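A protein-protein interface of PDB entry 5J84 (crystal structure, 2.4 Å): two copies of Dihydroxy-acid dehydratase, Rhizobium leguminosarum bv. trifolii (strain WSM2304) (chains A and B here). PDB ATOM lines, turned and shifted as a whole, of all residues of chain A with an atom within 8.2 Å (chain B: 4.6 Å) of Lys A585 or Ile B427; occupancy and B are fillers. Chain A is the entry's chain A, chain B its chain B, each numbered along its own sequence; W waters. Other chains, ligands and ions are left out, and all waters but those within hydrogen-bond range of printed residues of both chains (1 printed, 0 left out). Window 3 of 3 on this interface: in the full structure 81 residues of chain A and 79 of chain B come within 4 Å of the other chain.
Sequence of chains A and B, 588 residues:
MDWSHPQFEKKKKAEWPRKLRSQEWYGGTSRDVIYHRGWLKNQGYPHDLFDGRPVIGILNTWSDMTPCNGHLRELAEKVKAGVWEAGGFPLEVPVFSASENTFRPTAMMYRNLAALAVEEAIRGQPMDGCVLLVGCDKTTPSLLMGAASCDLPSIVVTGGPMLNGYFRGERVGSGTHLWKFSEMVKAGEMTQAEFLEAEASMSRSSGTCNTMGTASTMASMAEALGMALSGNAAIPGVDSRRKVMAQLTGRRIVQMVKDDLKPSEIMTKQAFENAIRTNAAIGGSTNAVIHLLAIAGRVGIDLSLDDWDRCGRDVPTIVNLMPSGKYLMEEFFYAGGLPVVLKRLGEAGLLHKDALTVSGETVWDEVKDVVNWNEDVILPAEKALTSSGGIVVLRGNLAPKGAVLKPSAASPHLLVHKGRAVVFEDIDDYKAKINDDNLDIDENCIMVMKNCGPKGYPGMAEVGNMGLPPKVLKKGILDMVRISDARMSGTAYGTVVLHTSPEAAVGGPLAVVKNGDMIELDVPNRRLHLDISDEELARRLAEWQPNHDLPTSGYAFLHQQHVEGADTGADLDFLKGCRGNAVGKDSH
Arg B104 touches Trp A25 (CD to NE1, 3.2 Å).
CG1 of Val A583 touches NH2 of Arg B104 (3.8 Å).
Pro B105 touches Gly A584 (N to CA, 3.99 Å).
Ile B427 touches Lys A585 (CG2 to NZ, 3.3 Å).
Asp A586 touches Pro B105 (O to O, 3.6 Å).
CA of Ser A587 touches O of Pro B105 (3.4 Å).
His A588 touches Val B463 (OXT to CG1, 3.6 Å).
Printed residues of chain B within 4 Å of Trp A25: Arg B104.
Arg A31 touches none of the printed residues of chain B.
Of the printed residues of chain B, Lys A585 touches Arg B104 (3.2 Å), Pro B105 (3.0 Å), Ile B427 (3.3 Å) and Tyr B457 (3.1 Å).
Of the printed residues of chain B, Asp A586 touches Arg B104, Pro B105 and Tyr B457.
Of the printed residues of chain A, Arg B104 touches Trp A25, Gly A124, Val A583, Gly A584, Lys A585 and Asp A586.
Asp B426 touches none of the printed residues of chain A.
Ile B427 touches just one residue of chain A: Lys A585 (3.3 Å).
The nearest printed residue of chain B that does not touch Lys A585 is Asp B428 (5.0 Å).
The guanidinium group (NH2) of Arg A31 is in salt-bridge range of the chain-end carboxylate (OXT) of His A588 (3.2 Å).
NE2 of His A36 lies within hydrogen-bond range of OD1 of Asp A586, 3.1 Å away.
The side-chain hydroxyl of Ser A587 lies within hydrogen-bond range of a ring nitrogen (ND1) of His A588 (3.0 Å).
Hydrophobic or aromatic side chains of chain B that line the printed part of chain A: Pro B105, Ile B427, Tyr B457 and Val B463.
Among the printed residues, 15 pairs touch across the chains.
Among the printed residues, Asp or Glu carboxylates within 4 Å of a Lys or Arg side-chain nitrogen of the other chain: Asp A586 with Arg B104 (3.2 Å).
N of Arg B104 lies within hydrogen-bond range of O of Gly A124.
The backbone carbonyl oxygen (O) of Gly A584 is in hydrogen-bond range of the guanidinium group (NH2) of Arg B104 (3.1 Å).
The backbone carbonyl oxygen (O) of Lys A585 sits at hydrogen-bond distance from the guanidinium group (NE) of Arg B104 (3.2 Å).
The backbone carbonyl oxygen of Tyr B457 is in hydrogen-bond range of the side-chain amino group of Lys A585 (3.1 Å).
The side-chain carboxylate of Asp A586 lies within salt-bridge range of the guanidinium group of Arg B104, 3.2 Å away.
The side-chain hydroxyl of Tyr B457 lies within hydrogen-bond range of the backbone carbonyl oxygen of Asp A586 (3.1 Å).
The chain-end carboxylate of His A588 lies within salt-bridge range of the side-chain amino group of Lys B431 (3.9 Å).
The backbone carbonyl oxygen (O) of Pro B105 lies close to the backbone carbonyl oxygen (O) of Lys A585 (3.1 Å).
No position is printed for both chains.
Of the 15 pairs that touch across the chains among the printed residues, none has its exchanged pair printed and touching as well.
Water W1 bridges O of Val B463 (3.3 Å) and OXT of His A588 (3.5 Å).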
ATOM      1  N   TRP A  25      36.262  -2.270  10.381  1.00  0.00           N
ATOM      2  CA  TRP A  25      35.306  -3.330  10.088  1.00  0.00           C
ATOM      3  C   TRP A  25      35.876  -4.730  10.314  1.00  0.00           C
ATOM      4  O   TRP A  25      35.198  -5.604  10.850  1.00  0.00           O
ATOM      5  CB  TRP A  25      34.835  -3.231   8.637  1.00  0.00           C
ATOM      6  CG  TRP A  25      33.860  -2.136   8.339  1.00  0.00           C
ATOM      7  CD1 TRP A  25      32.504  -2.246   8.267  1.00  0.00           C
ATOM      8  CD2 TRP A  25      34.170  -0.770   8.031  1.00  0.00           C
ATOM      9  NE1 TRP A  25      31.948  -1.033   7.942  1.00  0.00           N
ATOM     10  CE2 TRP A  25      32.950  -0.111   7.792  1.00  0.00           C
ATOM     11  CE3 TRP A  25      35.360  -0.043   7.937  1.00  0.00           C
ATOM     12  CZ2 TRP A  25      32.885   1.241   7.471  1.00  0.00           C
ATOM     13  CZ3 TRP A  25      35.292   1.295   7.612  1.00  0.00           C
ATOM     14  CH2 TRP A  25      34.065   1.923   7.383  1.00  0.00           C
ATOM     15  N   ARG A  31      32.459  -8.648  18.392  1.00  0.00           N
ATOM     16  CA  ARG A  31      31.248  -9.131  17.741  1.00  0.00           C
ATOM     17  C   ARG A  31      31.049  -8.444  16.392  1.00  0.00           C
ATOM     18  O   ARG A  31      30.639  -9.077  15.420  1.00  0.00           O
ATOM     19  CB  ARG A  31      30.023  -8.924  18.643  1.00  0.00           C
ATOM     20  CG  ARG A  31      28.712  -9.392  18.014  1.00  0.00           C
ATOM     21  CD  ARG A  31      27.478  -8.922  18.782  1.00  0.00           C
ATOM     22  NE  ARG A  31      27.306  -7.472  18.763  1.00  0.00           N
ATOM     23  CZ  ARG A  31      26.453  -6.814  19.543  1.00  0.00           C
ATOM     24  NH1 ARG A  31      25.688  -7.477  20.400  1.00  0.00           N
ATOM     25  NH2 ARG A  31      26.360  -5.494  19.462  1.00  0.00           N
ATOM     26  N   ASP A  32      31.351  -7.149  16.336  1.00  0.00           N
ATOM     27  CA  ASP A  32      31.153  -6.377  15.116  1.00  0.00           C
ATOM     28  C   ASP A  32      32.059  -6.880  14.003  1.00  0.00           C
ATOM     29  O   ASP A  32      31.649  -6.963  12.848  1.00  0.00           O
ATOM     30  CB  ASP A  32      31.427  -4.892  15.358  1.00  0.00           C
ATOM     31  CG  ASP A  32      30.434  -4.260  16.307  1.00  0.00           C
ATOM     32  OD1 ASP A  32      29.244  -4.641  16.266  1.00  0.00           O
ATOM     33  OD2 ASP A  32      30.843  -3.372  17.086  1.00  0.00           O
ATOM     34  N   HIS A  36      31.067  -8.471  10.376  1.00  0.00           N
ATOM     35  CA  HIS A  36      31.546  -7.890   9.128  1.00  0.00           C
ATOM     36  C   HIS A  36      32.415  -8.866   8.338  1.00  0.00           C
ATOM     37  O   HIS A  36      32.159  -9.121   7.160  1.00  0.00           O
ATOM     38  CB  HIS A  36      32.331  -6.602   9.400  1.00  0.00           C
ATOM     39  CG  HIS A  36      31.499  -5.484   9.948  1.00  0.00           C
ATOM     40  ND1 HIS A  36      30.336  -5.054   9.343  1.00  0.00           N
ATOM     41  CD2 HIS A  36      31.671  -4.689  11.030  1.00  0.00           C
ATOM     42  CE1 HIS A  36      29.822  -4.056  10.037  1.00  0.00           C
ATOM     43  NE2 HIS A  36      30.615  -3.814  11.068  1.00  0.00           N
ATOM     44  N   GLY A 124      30.898   5.462   3.754  1.00  0.00           N
ATOM     45  CA  GLY A 124      30.089   4.533   4.525  1.00  0.00           C
ATOM     46  C   GLY A 124      30.545   3.084   4.548  1.00  0.00           C
ATOM     47  O   GLY A 124      30.072   2.299   5.364  1.00  0.00           O
ATOM     48  N   ALA A 582      35.869  10.092   7.868  1.00  0.00           N
ATOM     49  CA  ALA A 582      35.759   9.455   9.175  1.00  0.00           C
ATOM     50  C   ALA A 582      34.730   8.331   9.147  1.00  0.00           C
ATOM     51  O   ALA A 582      33.629   8.493   8.620  1.00  0.00           O
ATOM     52  CB  ALA A 582      35.401  10.481  10.244  1.00  0.00           C
ATOM     53  N   VAL A 583      35.098   7.196   9.726  1.00  0.00           N
ATOM     54  CA  VAL A 583      34.221   6.034   9.776  1.00  0.00           C
ATOM     55  C   VAL A 583      33.035   6.292  10.694  1.00  0.00           C
ATOM     56  O   VAL A 583      33.201   6.770  11.816  1.00  0.00           O
ATOM     57  CB  VAL A 583      34.984   4.786  10.266  1.00  0.00           C
ATOM     58  CG1 VAL A 583      34.060   3.586  10.372  1.00  0.00           C
ATOM     59  CG2 VAL A 583      36.171   4.496   9.357  1.00  0.00           C
ATOM     60  N   GLY A 584      31.835   5.977  10.216  1.00  0.00           N
ATOM     61  CA  GLY A 584      30.644   6.204  11.008  1.00  0.00           C
ATOM     62  C   GLY A 584      30.558   5.208  12.147  1.00  0.00           C
ATOM     63  O   GLY A 584      31.383   4.299  12.255  1.00  0.00           O
ATOM     64  N   LYS A 585      29.558   5.384  13.002  1.00  0.00           N
ATOM     65  CA  LYS A 585      29.321   4.479  14.119  1.00  0.00           C
ATOM     66  C   LYS A 585      29.029   3.069  13.626  1.00  0.00           C
ATOM     67  O   LYS A 585      28.605   2.881  12.492  1.00  0.00           O
ATOM     68  CB  LYS A 585      28.162   5.001  14.964  1.00  0.00           C
ATOM     69  CG  LYS A 585      28.464   6.328  15.637  1.00  0.00           C
ATOM     70  CD  LYS A 585      27.200   6.998  16.138  1.00  0.00           C
ATOM     71  CE  LYS A 585      26.741   6.406  17.450  1.00  0.00           C
ATOM     72  NZ  LYS A 585      25.484   7.051  17.922  1.00  0.00           N
ATOM     73  N   ASP A 586      29.268   2.071  14.468  1.00  0.00           N
ATOM     74  CA  ASP A 586      28.971   0.700  14.083  1.00  0.00           C
ATOM     75  C   ASP A 586      27.455   0.525  14.043  1.00  0.00           C
ATOM     76  O   ASP A 586      26.723   1.268  14.698  1.00  0.00           O
ATOM     77  CB  ASP A 586      29.630  -0.306  15.024  1.00  0.00           C
ATOM     78  CG  ASP A 586      30.284  -1.458  14.273  1.00  0.00           C
ATOM     79  OD1 ASP A 586      29.662  -1.996  13.330  1.00  0.00           O
ATOM     80  OD2 ASP A 586      31.431  -1.814  14.614  1.00  0.00           O
ATOM     81  N   SER A 587      26.983  -0.444  13.266  1.00  0.00           N
ATOM     82  CA  SER A 587      25.551  -0.596  13.030  1.00  0.00           C
ATOM     83  C   SER A 587      24.845  -1.312  14.183  1.00  0.00           C
ATOM     84  O   SER A 587      23.619  -1.268  14.288  1.00  0.00           O
ATOM     85  CB  SER A 587      25.304  -1.346  11.716  1.00  0.00           C
ATOM     86  OG  SER A 587      26.039  -2.557  11.662  1.00  0.00           O
ATOM     87  N   HIS A 588      25.617  -1.960  15.051  1.00  0.00           N
ATOM     88  CA  HIS A 588      25.043  -2.669  16.193  1.00  0.00           C
ATOM     89  C   HIS A 588      25.820  -2.367  17.473  1.00  0.00           C
ATOM     90  O   HIS A 588      26.951  -1.883  17.435  1.00  0.00           O
ATOM     91  CB  HIS A 588      25.025  -4.182  15.945  1.00  0.00           C
ATOM     92  CG  HIS A 588      24.216  -4.596  14.753  1.00  0.00           C
ATOM     93  ND1 HIS A 588      24.701  -4.530  13.464  1.00  0.00           N
ATOM     94  CD2 HIS A 588      22.954  -5.078  14.656  1.00  0.00           C
ATOM     95  CE1 HIS A 588      23.774  -4.958  12.625  1.00  0.00           C
ATOM     96  NE2 HIS A 588      22.705  -5.297  13.323  1.00  0.00           N
ATOM     97  OXT HIS A 588      25.331  -2.600  18.579  1.00  0.00           O
ATOM     98  N   ARG B 104      28.152   1.976   7.343  1.00  0.00           N
ATOM     99  CA  ARG B 104      28.162   2.645   8.637  1.00  0.00           C
ATOM    100  C   ARG B 104      28.025   4.152   8.428  1.00  0.00           C
ATOM    101  O   ARG B 104      28.583   4.693   7.474  1.00  0.00           O
ATOM    102  CB  ARG B 104      29.424   2.292   9.421  1.00  0.00           C
ATOM    103  CG  ARG B 104      29.363   0.889  10.011  1.00  0.00           C
ATOM    104  CD  ARG B 104      30.707   0.414  10.528  1.00  0.00           C
ATOM    105  NE  ARG B 104      31.232   1.240  11.608  1.00  0.00           N
ATOM    106  CZ  ARG B 104      32.252   0.881  12.378  1.00  0.00           C
ATOM    107  NH1 ARG B 104      32.850  -0.287  12.181  1.00  0.00           N
ATOM    108  NH2 ARG B 104      32.676   1.687  13.342  1.00  0.00           N
ATOM    109  N   PRO B 105      27.296   4.847   9.325  1.00  0.00           N
ATOM    110  CA  PRO B 105      26.749   4.404  10.620  1.00  0.00           C
ATOM    111  C   PRO B 105      25.701   3.287  10.571  1.00  0.00           C
ATOM    112  O   PRO B 105      25.720   2.421  11.447  1.00  0.00           O
ATOM    113  CB  PRO B 105      26.124   5.687  11.185  1.00  0.00           C
ATOM    114  CG  PRO B 105      25.818   6.516   9.991  1.00  0.00           C
ATOM    115  CD  PRO B 105      26.929   6.244   9.028  1.00  0.00           C
ATOM    116  N   ASP B 426      22.369   7.778  25.355  1.00  0.00           N
ATOM    117  CA  ASP B 426      22.718   7.398  23.986  1.00  0.00           C
ATOM    118  C   ASP B 426      23.463   6.064  23.976  1.00  0.00           C
ATOM    119  O   ASP B 426      23.648   5.446  25.024  1.00  0.00           O
ATOM    120  CB  ASP B 426      23.565   8.484  23.311  1.00  0.00           C
ATOM    121  CG  ASP B 426      24.755   8.918  24.155  1.00  0.00           C
ATOM    122  OD1 ASP B 426      25.379   8.063  24.821  1.00  0.00           O
ATOM    123  OD2 ASP B 426      25.069  10.128  24.153  1.00  0.00           O
ATOM    124  N   ILE B 427      23.887   5.623  22.795  1.00  0.00           N
ATOM    125  CA  ILE B 427      24.560   4.334  22.658  1.00  0.00           C
ATOM    126  C   ILE B 427      25.939   4.339  23.325  1.00  0.00           C
ATOM    127  O   ILE B 427      26.404   3.309  23.813  1.00  0.00           O
ATOM    128  CB  ILE B 427      24.702   3.923  21.172  1.00  0.00           C
ATOM    129  CG1 ILE B 427      25.242   2.496  21.057  1.00  0.00           C
ATOM    130  CG2 ILE B 427      25.600   4.885  20.423  1.00  0.00           C
ATOM    131  CD1 ILE B 427      24.308   1.447  21.606  1.00  0.00           C
ATOM    132  N   ASP B 428      26.574   5.506  23.369  1.00  0.00           N
ATOM    133  CA  ASP B 428      27.870   5.640  24.022  1.00  0.00           C
ATOM    134  C   ASP B 428      27.698   5.461  25.519  1.00  0.00           C
ATOM    135  O   ASP B 428      28.528   4.842  26.184  1.00  0.00           O
ATOM    136  CB  ASP B 428      28.500   7.000  23.720  1.00  0.00           C
ATOM    137  CG  ASP B 428      28.882   7.154  22.264  1.00  0.00           C
ATOM    138  OD1 ASP B 428      29.376   6.170  21.674  1.00  0.00           O
ATOM    139  OD2 ASP B 428      28.696   8.259  21.712  1.00  0.00           O
ATOM    140  N   ASP B 429      26.608   6.016  26.035  1.00  0.00           N
ATOM    141  CA  ASP B 429      26.269   5.887  27.443  1.00  0.00           C
ATOM    142  C   ASP B 429      26.083   4.417  27.805  1.00  0.00           C
ATOM    143  O   ASP B 429      26.626   3.943  28.801  1.00  0.00           O
ATOM    144  CB  ASP B 429      25.002   6.684  27.760  1.00  0.00           C
ATOM    145  CG  ASP B 429      24.852   6.975  29.237  1.00  0.00           C
ATOM    146  OD1 ASP B 429      25.886   7.160  29.911  1.00  0.00           O
ATOM    147  OD2 ASP B 429      23.702   7.020  29.722  1.00  0.00           O
ATOM    148  N   TYR B 430      25.318   3.703  26.984  1.00  0.00           N
ATOM    149  CA  TYR B 430      25.079   2.276  27.189  1.00  0.00           C
ATOM    150  C   TYR B 430      26.357   1.447  27.265  1.00  0.00           C
ATOM    151  O   TYR B 430      26.554   0.694  28.216  1.00  0.00           O
ATOM    152  CB  TYR B 430      24.189   1.724  26.072  1.00  0.00           C
ATOM    153  CG  TYR B 430      24.224   0.214  25.957  1.00  0.00           C
ATOM    154  CD1 TYR B 430      23.526  -0.588  26.851  1.00  0.00           C
ATOM    155  CD2 TYR B 430      24.959  -0.408  24.955  1.00  0.00           C
ATOM    156  CE1 TYR B 430      23.558  -1.967  26.748  1.00  0.00           C
ATOM    157  CE2 TYR B 430      24.999  -1.785  24.845  1.00  0.00           C
ATOM    158  CZ  TYR B 430      24.298  -2.560  25.744  1.00  0.00           C
ATOM    159  OH  TYR B 430      24.335  -3.932  25.637  1.00  0.00           O
ATOM    160  N   LYS B 431      27.224   1.582  26.266  1.00  0.00           N
ATOM    161  CA  LYS B 431      28.447   0.787  26.232  1.00  0.00           C
ATOM    162  C   LYS B 431      29.400   1.159  27.367  1.00  0.00           C
ATOM    163  O   LYS B 431      30.239   0.355  27.768  1.00  0.00           O
ATOM    164  CB  LYS B 431      29.145   0.903  24.876  1.00  0.00           C
ATOM    165  CG  LYS B 431      28.479   0.051  23.801  1.00  0.00           C
ATOM    166  CD  LYS B 431      29.308  -0.039  22.532  1.00  0.00           C
ATOM    167  CE  LYS B 431      28.673  -1.016  21.546  1.00  0.00           C
ATOM    168  NZ  LYS B 431      29.491  -1.208  20.315  1.00  0.00           N
ATOM    169  N   MET B 449      16.985   3.360  26.539  1.00  0.00           N
ATOM    170  CA  MET B 449      18.011   4.126  25.844  1.00  0.00           C
ATOM    171  C   MET B 449      17.369   5.072  24.843  1.00  0.00           C
ATOM    172  O   MET B 449      16.402   4.713  24.178  1.00  0.00           O
ATOM    173  CB  MET B 449      18.999   3.201  25.136  1.00  0.00           C
ATOM    174  CG  MET B 449      20.111   3.934  24.406  1.00  0.00           C
ATOM    175  SD  MET B 449      21.473   2.848  23.955  1.00  0.00           S
ATOM    176  CE  MET B 449      20.627   1.683  22.891  1.00  0.00           C
ATOM    177  N   CYS B 452      18.685   7.232  19.581  1.00  0.00           N
ATOM    178  CA  CYS B 452      19.157   6.214  18.652  1.00  0.00           C
ATOM    179  C   CYS B 452      18.172   6.052  17.496  1.00  0.00           C
ATOM    180  O   CYS B 452      18.178   5.041  16.796  1.00  0.00           O
ATOM    181  CB  CYS B 452      19.365   4.877  19.364  1.00  0.00           C
ATOM    182  SG  CYS B 452      20.643   4.894  20.638  1.00  0.00           S
ATOM    183  N   TYR B 457      20.583   9.063  16.040  1.00  0.00           N
ATOM    184  CA  TYR B 457      21.772   8.213  16.065  1.00  0.00           C
ATOM    185  C   TYR B 457      22.962   8.771  15.264  1.00  0.00           C
ATOM    186  O   TYR B 457      24.063   8.862  15.801  1.00  0.00           O
ATOM    187  CB  TYR B 457      21.430   6.800  15.575  1.00  0.00           C
ATOM    188  CG  TYR B 457      22.494   5.780  15.913  1.00  0.00           C
ATOM    189  CD1 TYR B 457      22.513   5.163  17.157  1.00  0.00           C
ATOM    190  CD2 TYR B 457      23.486   5.446  15.002  1.00  0.00           C
ATOM    191  CE1 TYR B 457      23.482   4.235  17.483  1.00  0.00           C
ATOM    192  CE2 TYR B 457      24.461   4.517  15.318  1.00  0.00           C
ATOM    193  CZ  TYR B 457      24.454   3.915  16.561  1.00  0.00           C
ATOM    194  OH  TYR B 457      25.418   2.991  16.886  1.00  0.00           O
ATOM    195  N   VAL B 463      20.217  -1.248  17.540  1.00  0.00           N
ATOM    196  CA  VAL B 463      20.827  -1.392  18.859  1.00  0.00           C
ATOM    197  C   VAL B 463      19.770  -1.585  19.935  1.00  0.00           C
ATOM    198  O   VAL B 463      20.059  -1.467  21.127  1.00  0.00           O
ATOM    199  CB  VAL B 463      21.685  -0.165  19.229  1.00  0.00           C
ATOM    200  CG1 VAL B 463      22.868  -0.043  18.286  1.00  0.00           C
ATOM    201  CG2 VAL B 463      20.843   1.102  19.205  1.00  0.00           C
HETATM  202  O   HOH W   1      23.160  -2.464  21.257  1.00  0.00           O
